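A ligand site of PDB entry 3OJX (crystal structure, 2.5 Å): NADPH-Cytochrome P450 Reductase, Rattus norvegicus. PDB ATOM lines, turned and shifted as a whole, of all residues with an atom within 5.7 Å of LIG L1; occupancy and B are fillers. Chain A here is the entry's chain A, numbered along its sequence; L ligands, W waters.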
ATOM      1  N   GLY A  29     -22.877  39.380  -1.218  1.00  0.00           N
ATOM      2  CA  GLY A  29     -22.143  39.233   0.018  1.00  0.00           C
ATOM      3  C   GLY A  29     -21.516  37.863  -0.167  1.00  0.00           C
ATOM      4  O   GLY A  29     -22.136  36.850   0.133  1.00  0.00           O
ATOM      5  N   SER A  30     -20.300  37.843  -0.677  1.00  0.00           N
ATOM      6  CA  SER A  30     -19.634  36.576  -0.951  1.00  0.00           C
ATOM      7  C   SER A  30     -18.153  36.566  -0.565  1.00  0.00           C
ATOM      8  O   SER A  30     -17.522  37.610  -0.505  1.00  0.00           O
ATOM      9  CB  SER A  30     -19.788  36.269  -2.450  1.00  0.00           C
ATOM     10  OG  SER A  30     -19.056  35.124  -2.844  1.00  0.00           O
ATOM     11  N   GLN A  31     -17.624  35.366  -0.302  1.00  0.00           N
ATOM     12  CA  GLN A  31     -16.224  35.222   0.067  1.00  0.00           C
ATOM     13  C   GLN A  31     -15.493  34.188  -0.813  1.00  0.00           C
ATOM     14  O   GLN A  31     -14.275  34.272  -0.967  1.00  0.00           O
ATOM     15  CB  GLN A  31     -16.123  34.838   1.565  1.00  0.00           C
ATOM     16  CG  GLN A  31     -14.801  35.283   2.207  1.00  0.00           C
ATOM     17  CD  GLN A  31     -14.780  35.135   3.740  1.00  0.00           C
ATOM     18  OE1 GLN A  31     -15.520  35.816   4.464  1.00  0.00           O
ATOM     19  NE2 GLN A  31     -13.912  34.262   4.219  1.00  0.00           N
ATOM     20  N   THR A  32     -16.217  33.227  -1.384  1.00  0.00           N
ATOM     21  CA  THR A  32     -15.588  32.246  -2.264  1.00  0.00           C
ATOM     22  C   THR A  32     -16.231  32.229  -3.669  1.00  0.00           C
ATOM     23  O   THR A  32     -16.001  31.322  -4.450  1.00  0.00           O
ATOM     24  CB  THR A  32     -15.571  30.797  -1.676  1.00  0.00           C
ATOM     25  OG1 THR A  32     -16.898  30.368  -1.365  1.00  0.00           O
ATOM     26  CG2 THR A  32     -14.720  30.759  -0.409  1.00  0.00           C
ATOM     27  N   GLY A  33     -17.042  33.237  -3.959  1.00  0.00           N
ATOM     28  CA  GLY A  33     -17.654  33.344  -5.266  1.00  0.00           C
ATOM     29  C   GLY A  33     -19.051  32.812  -5.542  1.00  0.00           C
ATOM     30  O   GLY A  33     -19.656  33.186  -6.549  1.00  0.00           O
ATOM     31  N   THR A  34     -19.590  31.957  -4.679  1.00  0.00           N
ATOM     32  CA  THR A  34     -20.929  31.434  -4.967  1.00  0.00           C
ATOM     33  C   THR A  34     -21.960  32.549  -5.094  1.00  0.00           C
ATOM     34  O   THR A  34     -22.568  32.696  -6.157  1.00  0.00           O
ATOM     35  CB  THR A  34     -21.379  30.406  -3.907  1.00  0.00           C
ATOM     36  OG1 THR A  34     -20.274  29.552  -3.556  1.00  0.00           O
ATOM     37  CG2 THR A  34     -22.518  29.559  -4.464  1.00  0.00           C
ATOM     38  N   ALA A  35     -22.157  33.350  -4.051  1.00  0.00           N
ATOM     39  CA  ALA A  35     -23.136  34.430  -4.115  1.00  0.00           C
ATOM     40  C   ALA A  35     -22.802  35.428  -5.228  1.00  0.00           C
ATOM     41  O   ALA A  35     -23.690  36.027  -5.837  1.00  0.00           O
ATOM     42  CB  ALA A  35     -23.196  35.159  -2.785  1.00  0.00           C
ATOM     43  N   GLU A  36     -21.510  35.619  -5.493  1.00  0.00           N
ATOM     44  CA  GLU A  36     -21.099  36.544  -6.539  1.00  0.00           C
ATOM     45  C   GLU A  36     -21.664  36.092  -7.883  1.00  0.00           C
ATOM     46  O   GLU A  36     -22.248  36.889  -8.624  1.00  0.00           O
ATOM     47  CB  GLU A  36     -19.570  36.646  -6.614  1.00  0.00           C
ATOM     48  CG  GLU A  36     -19.103  37.488  -7.801  1.00  0.00           C
ATOM     49  CD  GLU A  36     -17.597  37.720  -7.825  1.00  0.00           C
ATOM     50  OE1 GLU A  36     -16.847  36.908  -7.229  1.00  0.00           O
ATOM     51  OE2 GLU A  36     -17.163  38.711  -8.472  1.00  0.00           O
ATOM     52  N   ALA A  82     -23.949  35.495   1.619  1.00  0.00           N
ATOM     53  CA  ALA A  82     -23.477  34.249   2.218  1.00  0.00           C
ATOM     54  C   ALA A  82     -23.268  34.473   3.727  1.00  0.00           C
ATOM     55  O   ALA A  82     -22.985  35.586   4.159  1.00  0.00           O
ATOM     56  CB  ALA A  82     -22.189  33.803   1.577  1.00  0.00           C
ATOM     57  N   THR A  83     -23.421  33.424   4.519  1.00  0.00           N
ATOM     58  CA  THR A  83     -23.233  33.522   5.959  1.00  0.00           C
ATOM     59  C   THR A  83     -21.972  32.773   6.401  1.00  0.00           C
ATOM     60  O   THR A  83     -21.732  31.665   5.928  1.00  0.00           O
ATOM     61  CB  THR A  83     -24.441  32.922   6.713  1.00  0.00           C
ATOM     62  OG1 THR A  83     -25.607  33.724   6.466  1.00  0.00           O
ATOM     63  CG2 THR A  83     -24.178  32.884   8.206  1.00  0.00           C
ATOM     64  N   TYR A  84     -21.176  33.376   7.277  1.00  0.00           N
ATOM     65  CA  TYR A  84     -19.983  32.697   7.756  1.00  0.00           C
ATOM     66  C   TYR A  84     -19.953  32.506   9.259  1.00  0.00           C
ATOM     67  O   TYR A  84     -20.989  32.620   9.904  1.00  0.00           O
ATOM     68  CB  TYR A  84     -18.709  33.396   7.264  1.00  0.00           C
ATOM     69  CG  TYR A  84     -18.343  32.957   5.856  1.00  0.00           C
ATOM     70  CD1 TYR A  84     -19.158  33.296   4.765  1.00  0.00           C
ATOM     71  CD2 TYR A  84     -17.251  32.116   5.629  1.00  0.00           C
ATOM     72  CE1 TYR A  84     -18.908  32.797   3.490  1.00  0.00           C
ATOM     73  CE2 TYR A  84     -16.990  31.608   4.352  1.00  0.00           C
ATOM     74  CZ  TYR A  84     -17.829  31.957   3.293  1.00  0.00           C
ATOM     75  OH  TYR A  84     -17.597  31.431   2.030  1.00  0.00           O
ATOM     76  N   GLY A  85     -18.774  32.212   9.786  1.00  0.00           N
ATOM     77  CA  GLY A  85     -18.587  31.949  11.202  1.00  0.00           C
ATOM     78  C   GLY A  85     -19.499  32.602  12.221  1.00  0.00           C
ATOM     79  O   GLY A  85     -19.515  33.833  12.343  1.00  0.00           O
ATOM     80  N   GLU A  86     -20.233  31.797  12.977  1.00  0.00           N
ATOM     81  CA  GLU A  86     -21.124  32.321  14.003  1.00  0.00           C
ATOM     82  C   GLU A  86     -22.227  33.211  13.420  1.00  0.00           C
ATOM     83  O   GLU A  86     -22.850  33.994  14.146  1.00  0.00           O
ATOM     84  CB  GLU A  86     -20.350  33.159  15.025  1.00  0.00           C
ATOM     85  CG  GLU A  86     -19.326  32.410  15.868  1.00  0.00           C
ATOM     86  CD  GLU A  86     -18.671  33.310  16.915  1.00  0.00           C
ATOM     87  OE1 GLU A  86     -18.007  34.290  16.518  1.00  0.00           O
ATOM     88  OE2 GLU A  86     -18.824  33.032  18.127  1.00  0.00           O
ATOM     89  N   GLY A  87     -22.459  33.080  12.118  1.00  0.00           N
ATOM     90  CA  GLY A  87     -23.487  33.878  11.480  1.00  0.00           C
ATOM     91  C   GLY A  87     -23.043  35.265  11.030  1.00  0.00           C
ATOM     92  O   GLY A  87     -23.859  36.069  10.603  1.00  0.00           O
ATOM     93  N   THR A  90     -19.919  37.862   5.256  1.00  0.00           N
ATOM     94  CA  THR A  90     -18.683  37.635   4.532  1.00  0.00           C
ATOM     95  C   THR A  90     -17.859  38.922   4.756  1.00  0.00           C
ATOM     96  O   THR A  90     -18.388  39.924   5.215  1.00  0.00           O
ATOM     97  CB  THR A  90     -18.992  37.464   3.039  1.00  0.00           C
ATOM     98  OG1 THR A  90     -19.703  38.612   2.573  1.00  0.00           O
ATOM     99  CG2 THR A  90     -19.868  36.239   2.809  1.00  0.00           C
ATOM    100  N   LEU A 117     -27.225  32.526   1.087  1.00  0.00           N
ATOM    101  CA  LEU A 117     -26.508  31.260   0.948  1.00  0.00           C
ATOM    102  C   LEU A 117     -26.121  30.827   2.353  1.00  0.00           C
ATOM    103  O   LEU A 117     -25.544  31.616   3.110  1.00  0.00           O
ATOM    104  CB  LEU A 117     -25.233  31.421   0.104  1.00  0.00           C
ATOM    105  CG  LEU A 117     -25.385  31.873  -1.353  1.00  0.00           C
ATOM    106  CD1 LEU A 117     -25.879  33.331  -1.406  1.00  0.00           C
ATOM    107  CD2 LEU A 117     -24.053  31.744  -2.085  1.00  0.00           C
ATOM    108  N   GLY A 118     -26.449  29.578   2.706  1.00  0.00           N
ATOM    109  CA  GLY A 118     -26.121  29.052   4.022  1.00  0.00           C
ATOM    110  C   GLY A 118     -25.908  27.546   4.004  1.00  0.00           C
ATOM    111  O   GLY A 118     -25.706  26.971   2.941  1.00  0.00           O
ATOM    112  N   ASN A 119     -25.939  26.908   5.180  1.00  0.00           N
ATOM    113  CA  ASN A 119     -25.764  25.461   5.294  1.00  0.00           C
ATOM    114  C   ASN A 119     -26.347  25.005   6.627  1.00  0.00           C
ATOM    115  O   ASN A 119     -25.784  25.268   7.684  1.00  0.00           O
ATOM    116  CB  ASN A 119     -24.284  25.084   5.216  1.00  0.00           C
ATOM    117  CG  ASN A 119     -24.050  23.567   5.283  1.00  0.00           C
ATOM    118  OD1 ASN A 119     -24.529  22.884   6.195  1.00  0.00           O
ATOM    119  ND2 ASN A 119     -23.314  23.038   4.324  1.00  0.00           N
ATOM    120  N   LYS A 120     -27.485  24.325   6.572  1.00  0.00           N
ATOM    121  CA  LYS A 120     -28.163  23.866   7.781  1.00  0.00           C
ATOM    122  C   LYS A 120     -27.335  23.107   8.811  1.00  0.00           C
ATOM    123  O   LYS A 120     -27.756  22.999   9.971  1.00  0.00           O
ATOM    124  CB  LYS A 120     -29.376  23.025   7.382  1.00  0.00           C
ATOM    125  CG  LYS A 120     -30.469  23.788   6.628  1.00  0.00           C
ATOM    126  CD  LYS A 120     -31.665  22.888   6.302  1.00  0.00           C
ATOM    127  CE  LYS A 120     -32.706  23.625   5.473  1.00  0.00           C
ATOM    128  NZ  LYS A 120     -33.725  22.680   4.896  1.00  0.00           N
ATOM    129  N   TYR A 122     -24.597  24.007  10.155  1.00  0.00           N
ATOM    130  CA  TYR A 122     -23.959  24.952  11.071  1.00  0.00           C
ATOM    131  C   TYR A 122     -25.095  25.423  11.976  1.00  0.00           C
ATOM    132  O   TYR A 122     -26.258  25.224  11.642  1.00  0.00           O
ATOM    133  CB  TYR A 122     -23.365  26.134  10.313  1.00  0.00           C
ATOM    134  CG  TYR A 122     -22.167  25.792   9.451  1.00  0.00           C
ATOM    135  CD1 TYR A 122     -20.889  25.694   9.995  1.00  0.00           C
ATOM    136  CD2 TYR A 122     -22.318  25.540   8.086  1.00  0.00           C
ATOM    137  CE1 TYR A 122     -19.789  25.375   9.201  1.00  0.00           C
ATOM    138  CE2 TYR A 122     -21.228  25.222   7.281  1.00  0.00           C
ATOM    139  CZ  TYR A 122     -19.966  25.133   7.851  1.00  0.00           C
ATOM    140  OH  TYR A 122     -18.900  24.817   7.048  1.00  0.00           O
ATOM    141  N   GLU A 123     -24.793  26.053  13.106  1.00  0.00           N
ATOM    142  CA  GLU A 123     -25.868  26.489  13.992  1.00  0.00           C
ATOM    143  C   GLU A 123     -26.672  27.711  13.548  1.00  0.00           C
ATOM    144  O   GLU A 123     -27.901  27.735  13.694  1.00  0.00           O
ATOM    145  CB  GLU A 123     -25.328  26.737  15.405  1.00  0.00           C
ATOM    146  CG  GLU A 123     -24.851  25.462  16.090  1.00  0.00           C
ATOM    147  CD  GLU A 123     -24.683  25.619  17.590  1.00  0.00           C
ATOM    148  OE1 GLU A 123     -24.063  24.720  18.215  1.00  0.00           O
ATOM    149  OE2 GLU A 123     -25.176  26.631  18.150  1.00  0.00           O
ATOM    150  N   HIS A 124     -26.009  28.714  12.994  1.00  0.00           N
ATOM    151  CA  HIS A 124     -26.711  29.918  12.563  1.00  0.00           C
ATOM    152  C   HIS A 124     -27.010  29.895  11.066  1.00  0.00           C
ATOM    153  O   HIS A 124     -26.372  30.597  10.271  1.00  0.00           O
ATOM    154  CB  HIS A 124     -25.883  31.140  12.936  1.00  0.00           C
ATOM    155  CG  HIS A 124     -25.415  31.118  14.357  1.00  0.00           C
ATOM    156  ND1 HIS A 124     -26.283  31.134  15.419  1.00  0.00           N
ATOM    157  CD2 HIS A 124     -24.167  31.030  14.881  1.00  0.00           C
ATOM    158  CE1 HIS A 124     -25.596  31.049  16.550  1.00  0.00           C
ATOM    159  NE2 HIS A 124     -24.311  30.992  16.259  1.00  0.00           N
ATOM    160  N   PHE A 125     -27.994  29.088  10.697  1.00  0.00           N
ATOM    161  CA  PHE A 125     -28.393  28.932   9.313  1.00  0.00           C
ATOM    162  C   PHE A 125     -28.826  30.210   8.618  1.00  0.00           C
ATOM    163  O   PHE A 125     -29.851  30.802   8.950  1.00  0.00           O
ATOM    164  CB  PHE A 125     -29.513  27.894   9.226  1.00  0.00           C
ATOM    165  CG  PHE A 125     -29.920  27.583   7.834  1.00  0.00           C
ATOM    166  CD1 PHE A 125     -28.947  27.335   6.857  1.00  0.00           C
ATOM    167  CD2 PHE A 125     -31.271  27.502   7.486  1.00  0.00           C
ATOM    168  CE1 PHE A 125     -29.314  27.019   5.541  1.00  0.00           C
ATOM    169  CE2 PHE A 125     -31.651  27.180   6.172  1.00  0.00           C
ATOM    170  CZ  PHE A 125     -30.665  26.938   5.193  1.00  0.00           C
ATOM    171  N   ASN A 126     -28.040  30.649   7.641  1.00  0.00           N
ATOM    172  CA  ASN A 126     -28.347  31.859   6.869  1.00  0.00           C
ATOM    173  C   ASN A 126     -28.622  33.074   7.747  1.00  0.00           C
ATOM    174  O   ASN A 126     -29.494  33.883   7.424  1.00  0.00           O
ATOM    175  CB  ASN A 126     -29.554  31.604   5.958  1.00  0.00           C
ATOM    176  CG  ASN A 126     -29.151  31.253   4.536  1.00  0.00           C
ATOM    177  OD1 ASN A 126     -29.602  30.229   3.995  1.00  0.00           O
ATOM    178  ND2 ASN A 126     -28.325  32.091   3.929  1.00  0.00           N
ATOM    179  N   ALA A 127     -27.884  33.212   8.836  1.00  0.00           N
ATOM    180  CA  ALA A 127     -28.103  34.358   9.725  1.00  0.00           C
ATOM    181  C   ALA A 127     -27.978  35.680   8.964  1.00  0.00           C
ATOM    182  O   ALA A 127     -28.800  36.586   9.143  1.00  0.00           O
ATOM    183  CB  ALA A 127     -27.109  34.320  10.867  1.00  0.00           C
ATOM    184  N   ASP A 152     -26.334  24.851   1.250  1.00  0.00           N
ATOM    185  CA  ASP A 152     -25.222  24.145   0.633  1.00  0.00           C
ATOM    186  C   ASP A 152     -25.067  22.705   1.150  1.00  0.00           C
ATOM    187  O   ASP A 152     -24.218  21.954   0.664  1.00  0.00           O
ATOM    188  CB  ASP A 152     -23.933  24.952   0.832  1.00  0.00           C
ATOM    189  CG  ASP A 152     -22.874  24.639  -0.207  1.00  0.00           C
ATOM    190  OD1 ASP A 152     -23.220  24.327  -1.362  1.00  0.00           O
ATOM    191  OD2 ASP A 152     -21.668  24.728   0.127  1.00  0.00           O
ATOM    192  N   LEU A 156     -27.452  23.659  -3.145  1.00  0.00           N
ATOM    193  CA  LEU A 156     -27.605  25.104  -3.204  1.00  0.00           C
ATOM    194  C   LEU A 156     -28.072  25.615  -4.570  1.00  0.00           C
ATOM    195  O   LEU A 156     -29.024  26.395  -4.648  1.00  0.00           O
ATOM    196  CB  LEU A 156     -26.288  25.785  -2.807  1.00  0.00           C
ATOM    197  CG  LEU A 156     -26.278  27.312  -2.793  1.00  0.00           C
ATOM    198  CD1 LEU A 156     -27.402  27.838  -1.912  1.00  0.00           C
ATOM    199  CD2 LEU A 156     -24.922  27.789  -2.299  1.00  0.00           C
ATOM    200  N   VAL A 620     -14.107  30.253  13.025  1.00  0.00           N
ATOM    201  CA  VAL A 620     -14.231  29.027  12.238  1.00  0.00           C
ATOM    202  C   VAL A 620     -13.573  29.049  10.856  1.00  0.00           C
ATOM    203  O   VAL A 620     -13.798  29.951  10.058  1.00  0.00           O
ATOM    204  CB  VAL A 620     -15.734  28.626  12.132  1.00  0.00           C
ATOM    205  CG1 VAL A 620     -16.609  29.755  12.668  1.00  0.00           C
ATOM    206  CG2 VAL A 620     -16.099  28.282  10.700  1.00  0.00           C
ATOM    207  N   TRP A 621     -12.756  28.037  10.606  1.00  0.00           N
ATOM    208  CA  TRP A 621     -12.035  27.909   9.342  1.00  0.00           C
ATOM    209  C   TRP A 621     -12.751  27.015   8.331  1.00  0.00           C
ATOM    210  O   TRP A 621     -12.465  27.051   7.131  1.00  0.00           O
ATOM    211  CB  TRP A 621     -10.623  27.359   9.616  1.00  0.00           C
ATOM    212  CG  TRP A 621      -9.743  28.288  10.386  1.00  0.00           C
ATOM    213  CD1 TRP A 621     -10.098  29.478  10.946  1.00  0.00           C
ATOM    214  CD2 TRP A 621      -8.370  28.075  10.715  1.00  0.00           C
ATOM    215  NE1 TRP A 621      -9.019  30.032  11.603  1.00  0.00           N
ATOM    216  CE2 TRP A 621      -7.946  29.185  11.476  1.00  0.00           C
ATOM    217  CE3 TRP A 621      -7.448  27.053  10.449  1.00  0.00           C
ATOM    218  CZ2 TRP A 621      -6.642  29.299  11.980  1.00  0.00           C
ATOM    219  CZ3 TRP A 621      -6.153  27.167  10.943  1.00  0.00           C
ATOM    220  CH2 TRP A 621      -5.763  28.281  11.695  1.00  0.00           C
ATOM    221  N   SER A 622     -13.664  26.187   8.808  1.00  0.00           N
ATOM    222  CA  SER A 622     -14.400  25.308   7.909  1.00  0.00           C
ATOM    223  C   SER A 622     -15.684  24.822   8.579  1.00  0.00           C
ATOM    224  O   SER A 622     -15.861  25.080   9.797  1.00  0.00           O
ATOM    225  CB  SER A 622     -13.530  24.114   7.511  1.00  0.00           C
ATOM    226  OG  SER A 622     -13.158  23.351   8.645  1.00  0.00           O
ATOM    227  OXT SER A 622     -16.493  24.177   7.877  1.00  0.00           O
HETATM  228  N1  LIG L   1     -23.724  28.764   6.401  1.00  0.00           N
HETATM  229  C1  LIG L   1     -24.645  29.100   7.352  1.00  0.00           C
HETATM  230  O1  LIG L   1     -25.846  29.074   7.123  1.00  0.00           O
HETATM  231  N2  LIG L   1     -24.162  29.454   8.598  1.00  0.00           N
HETATM  232  C2  LIG L   1     -22.824  29.522   8.994  1.00  0.00           C
HETATM  233  O2  LIG L   1     -22.661  29.881  10.162  1.00  0.00           O
HETATM  234  C3  LIG L   1     -21.843  29.188   8.020  1.00  0.00           C
HETATM  235  N3  LIG L   1     -20.495  29.248   8.398  1.00  0.00           N
HETATM  236  C4  LIG L   1     -19.593  28.894   7.397  1.00  0.00           C
HETATM  237  C5  LIG L   1     -18.203  28.942   7.764  1.00  0.00           C
HETATM  238  C6  LIG L   1     -17.185  28.604   6.832  1.00  0.00           C
HETATM  239  C7  LIG L   1     -15.732  28.702   7.357  1.00  0.00           C
HETATM  240  C8  LIG L   1     -17.520  28.186   5.443  1.00  0.00           C
HETATM  241  C9  LIG L   1     -16.624  27.832   4.465  1.00  0.00           C
HETATM  242  C10 LIG L   1     -18.856  28.125   5.093  1.00  0.00           C
HETATM  243  C11 LIG L   1     -19.922  28.482   6.029  1.00  0.00           C
HETATM  244  N4  LIG L   1     -21.369  28.446   5.703  1.00  0.00           N
HETATM  245  C12 LIG L   1     -22.366  28.809   6.731  1.00  0.00           C
HETATM  246  C13 LIG L   1     -21.785  28.050   4.386  1.00  0.00           C
HETATM  247  C14 LIG L   1     -21.691  29.156   3.322  1.00  0.00           C
HETATM  248  O3  LIG L   1     -22.572  30.259   3.748  1.00  0.00           O
HETATM  249  C15 LIG L   1     -22.121  28.598   1.991  1.00  0.00           C
HETATM  250  O4  LIG L   1     -21.174  27.545   1.681  1.00  0.00           O
HETATM  251  C16 LIG L   1     -22.064  29.751   0.926  1.00  0.00           C
HETATM  252  O5  LIG L   1     -22.481  29.147  -0.064  1.00  0.00           O
HETATM  253  C17 LIG L   1     -20.681  30.254   0.565  1.00  0.00           C
HETATM  254  O6  LIG L   1     -20.798  31.367  -0.391  1.00  0.00           O
HETATM  255  P1  LIG L   1     -19.655  32.208  -1.094  1.00  0.00           P
HETATM  256  O7  LIG L   1     -18.953  31.384  -2.106  1.00  0.00           O
HETATM  257  O8  LIG L   1     -18.857  32.823   0.102  1.00  0.00           O
HETATM  258  O9  LIG L   1     -20.560  33.251  -1.908  1.00  0.00           O
HETATM  259  P1  LG2 L   2      -7.048  24.784  -2.071  1.00  0.00           P
HETATM  260  O1  LG2 L   2      -6.407  24.637  -3.379  1.00  0.00           O
HETATM  261  O2  LG2 L   2      -7.969  25.900  -1.937  1.00  0.00           O
HETATM  262  O3  LG2 L   2      -7.829  23.425  -1.674  1.00  0.00           O
HETATM  263  C1  LG2 L   2      -8.566  23.242  -0.426  1.00  0.00           C
HETATM  264  C2  LG2 L   2      -9.654  22.173  -0.580  1.00  0.00           C
HETATM  265  O4  LG2 L   2      -9.084  20.895  -0.856  1.00  0.00           O
HETATM  266  C3  LG2 L   2     -10.485  21.943   0.688  1.00  0.00           C
HETATM  267  O5  LG2 L   2     -11.503  22.933   0.848  1.00  0.00           O
HETATM  268  C4  LG2 L   2     -11.030  20.528   0.492  1.00  0.00           C
HETATM  269  O6  LG2 L   2     -12.282  20.482  -0.220  1.00  0.00           O
HETATM  270  C5  LG2 L   2      -9.894  19.864  -0.253  1.00  0.00           C
HETATM  271  N1  LG2 L   2      -8.978  18.984   0.540  1.00  0.00           N
HETATM  272  C6  LG2 L   2      -7.939  19.242   1.427  1.00  0.00           C
HETATM  273  N2  LG2 L   2      -7.269  18.189   2.004  1.00  0.00           N
HETATM  274  C7  LG2 L   2      -7.989  17.151   1.414  1.00  0.00           C
HETATM  275  C8  LG2 L   2      -7.898  15.712   1.507  1.00  0.00           C
HETATM  276  N3  LG2 L   2      -6.995  15.096   2.271  1.00  0.00           N
HETATM  277  N4  LG2 L   2      -8.784  14.904   0.764  1.00  0.00           N
HETATM  278  C9  LG2 L   2      -9.760  15.464  -0.064  1.00  0.00           C
HETATM  279  N5  LG2 L   2      -9.953  16.814  -0.248  1.00  0.00           N
HETATM  280  C10 LG2 L   2      -9.031  17.618   0.521  1.00  0.00           C
HETATM  281  N6  LG2 L   2      -5.454  27.722   6.960  1.00  0.00           N
HETATM  282  C11 LG2 L   2      -4.226  27.678   7.563  1.00  0.00           C
HETATM  283  O7  LG2 L   2      -3.421  26.810   7.206  1.00  0.00           O
HETATM  284  N7  LG2 L   2      -3.981  28.663   8.559  1.00  0.00           N
HETATM  285  C12 LG2 L   2      -4.885  29.682   8.997  1.00  0.00           C
HETATM  286  O8  LG2 L   2      -4.536  30.465   9.876  1.00  0.00           O
HETATM  287  C13 LG2 L   2      -6.196  29.670   8.321  1.00  0.00           C
HETATM  288  N8  LG2 L   2      -7.144  30.638   8.717  1.00  0.00           N
HETATM  289  C14 LG2 L   2      -8.407  30.628   8.065  1.00  0.00           C
HETATM  290  C15 LG2 L   2      -9.370  31.639   8.497  1.00  0.00           C
HETATM  291  C16 LG2 L   2     -10.699  31.742   7.941  1.00  0.00           C
HETATM  292  C17 LG2 L   2     -11.671  32.818   8.433  1.00  0.00           C
HETATM  293  C18 LG2 L   2     -11.071  30.743   6.846  1.00  0.00           C
HETATM  294  C19 LG2 L   2     -12.458  30.725   6.160  1.00  0.00           C
HETATM  295  C20 LG2 L   2     -10.151  29.779   6.419  1.00  0.00           C
HETATM  296  C21 LG2 L   2      -8.814  29.675   6.986  1.00  0.00           C
HETATM  297  N9  LG2 L   2      -7.777  28.684   6.605  1.00  0.00           N
HETATM  298  C22 LG2 L   2      -6.426  28.663   7.300  1.00  0.00           C
HETATM  299  C23 LG2 L   2      -7.927  27.648   5.540  1.00  0.00           C
HETATM  300  C24 LG2 L   2      -7.255  28.583   4.410  1.00  0.00           C
HETATM  301  O9  LG2 L   2      -8.036  29.745   4.014  1.00  0.00           O
HETATM  302  C25 LG2 L   2      -6.950  27.751   3.112  1.00  0.00           C
HETATM  303  O10 LG2 L   2      -8.215  27.257   2.678  1.00  0.00           O
HETATM  304  C26 LG2 L   2      -6.068  26.481   3.222  1.00  0.00           C
HETATM  305  O11 LG2 L   2      -4.814  26.948   3.663  1.00  0.00           O
HETATM  306  C27 LG2 L   2      -5.828  25.763   1.869  1.00  0.00           C
HETATM  307  O12 LG2 L   2      -5.800  26.592   0.760  1.00  0.00           O
HETATM  308  P2  LG2 L   2      -5.135  26.158  -0.596  1.00  0.00           P
HETATM  309  O13 LG2 L   2      -5.380  27.305  -1.503  1.00  0.00           O
HETATM  310  O14 LG2 L   2      -3.695  25.805  -0.403  1.00  0.00           O
HETATM  311  O15 LG2 L   2      -5.984  24.918  -0.945  1.00  0.00           O
HETATM  312  O   HOH W   1     -17.063  28.724   1.199  1.00  0.00           O
HETATM  313  O   HOH W   2     -20.330  29.477  11.838  1.00  0.00           O
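The side-chain hydroxyl (OG1) of Thr 83 is in hydrogen-bond range of the backbone NH (N) of Ala 127, at 3.3 Å.
O of Gly 29 is in hydrogen-bond range of N of Ala 82.
The backbone carbonyl oxygen (O) of Leu 117 is in hydrogen-bond range of the side-chain amide nitrogen (ND2) of Asn 126, 2.9 Å away.
OG1 of Thr 90 sits at hydrogen-bond distance from N of Ser 30 (3.4 Å).
The backbone carbonyl oxygen (O) of Gly 118 is in hydrogen-bond range of the backbone NH (N) of Asp 152 (2.8 Å).
The side-chain hydroxyl of Ser 30 is in hydrogen-bond range of the backbone NH of Gly 33 (3.0 Å).
The side-chain amide nitrogen (ND2) of Asn 126 lies close to the backbone NH (N) of Gly 118.
The side-chain hydroxyl (OH) of Tyr 122 sits at hydrogen-bond distance from the chain-end carboxylate (OXT) of Ser 622 (2.6 Å).
Merely in contact with LIG L1: Gly 118 (3.1 Å), Phe 125 (3.4 Å), Val 620 (3.4 Å), Ala 82 (3.4 Å), Tyr 122 (3.5 Å), Trp 621 (3.6 Å), Ser 622 (3.6 Å), Leu 156 (3.6 Å), Gly 85 (3.7 Å) and Gly 87 (3.8 Å).
Hydrophobic or aromatic side chains that line LIG L1: Ala 35, Ala 82, Tyr 84, Leu 117, Tyr 122, Phe 125, Leu 156 and Val 620.
The nearest printed residue that does not touch LIG L1 is Glu 86 (4.2 Å).
O of His 124 is in hydrogen-bond range of N2 of LIG L1 (3.0 Å).
O8 of LIG L1 lies within hydrogen-bond range of N of Thr 32, 3.1 Å away.
An oxygen (O9) of LIG L1 lies within hydrogen-bond range of the backbone NH of Ala 35.
O1 of LIG L1 lies within hydrogen-bond range of N of Asn 126 (2.8 Å).
The backbone carbonyl oxygen (O) of Leu 117 lies within hydrogen-bond range of an oxygen (O3) of LIG L1 (3.3 Å).
The backbone NH of Gly 33 is in hydrogen-bond range of an oxygen (O7) of LIG L1 (3.2 Å).
An oxygen (O8) of LIG L1 is in hydrogen-bond range of the backbone NH of Gln 31, at 2.9 Å.
The backbone NH (N) of Thr 34 lies within hydrogen-bond range of an oxygen (O7) of LIG L1, at 2.7 Å.
OD2 of Asp 152 sits at hydrogen-bond distance from O4 of LIG L1, at 3.3 Å.
OG of Ser 30 sits at hydrogen-bond distance from O9 of LIG L1 (2.6 Å).
An oxygen (O7) of LIG L1 is in hydrogen-bond range of the side-chain hydroxyl (OG1) of Thr 34, 2.7 Å away.
An oxygen (O3) of LIG L1 lies within hydrogen-bond range of the backbone carbonyl oxygen (O) of Thr 83 (2.7 Å).
OG1 of Thr 32 lies within hydrogen-bond range of O7 of LIG L1.
OH of Tyr 84 sits at hydrogen-bond distance from O8 of LIG L1, at 2.7 Å.
The backbone NH (N) of Asn 119 is in hydrogen-bond range of an oxygen (O1) of LIG L1 (2.9 Å).
O3 of LIG L1 is in hydrogen-bond range of N of Thr 83, 3.4 Å away.
N8 of LG2 L2 lies close to NE1 of Trp 621, 3.5 Å away.
Water W2 lies within hydrogen-bond range of the backbone NH of Glu 86 (2.6 Å) and an oxygen (O2) of LIG L1 (2.9 Å).
Water W1 bridges OH of Tyr 84 (2.9 Å) and OG1 of Thr 32 (3.1 Å).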
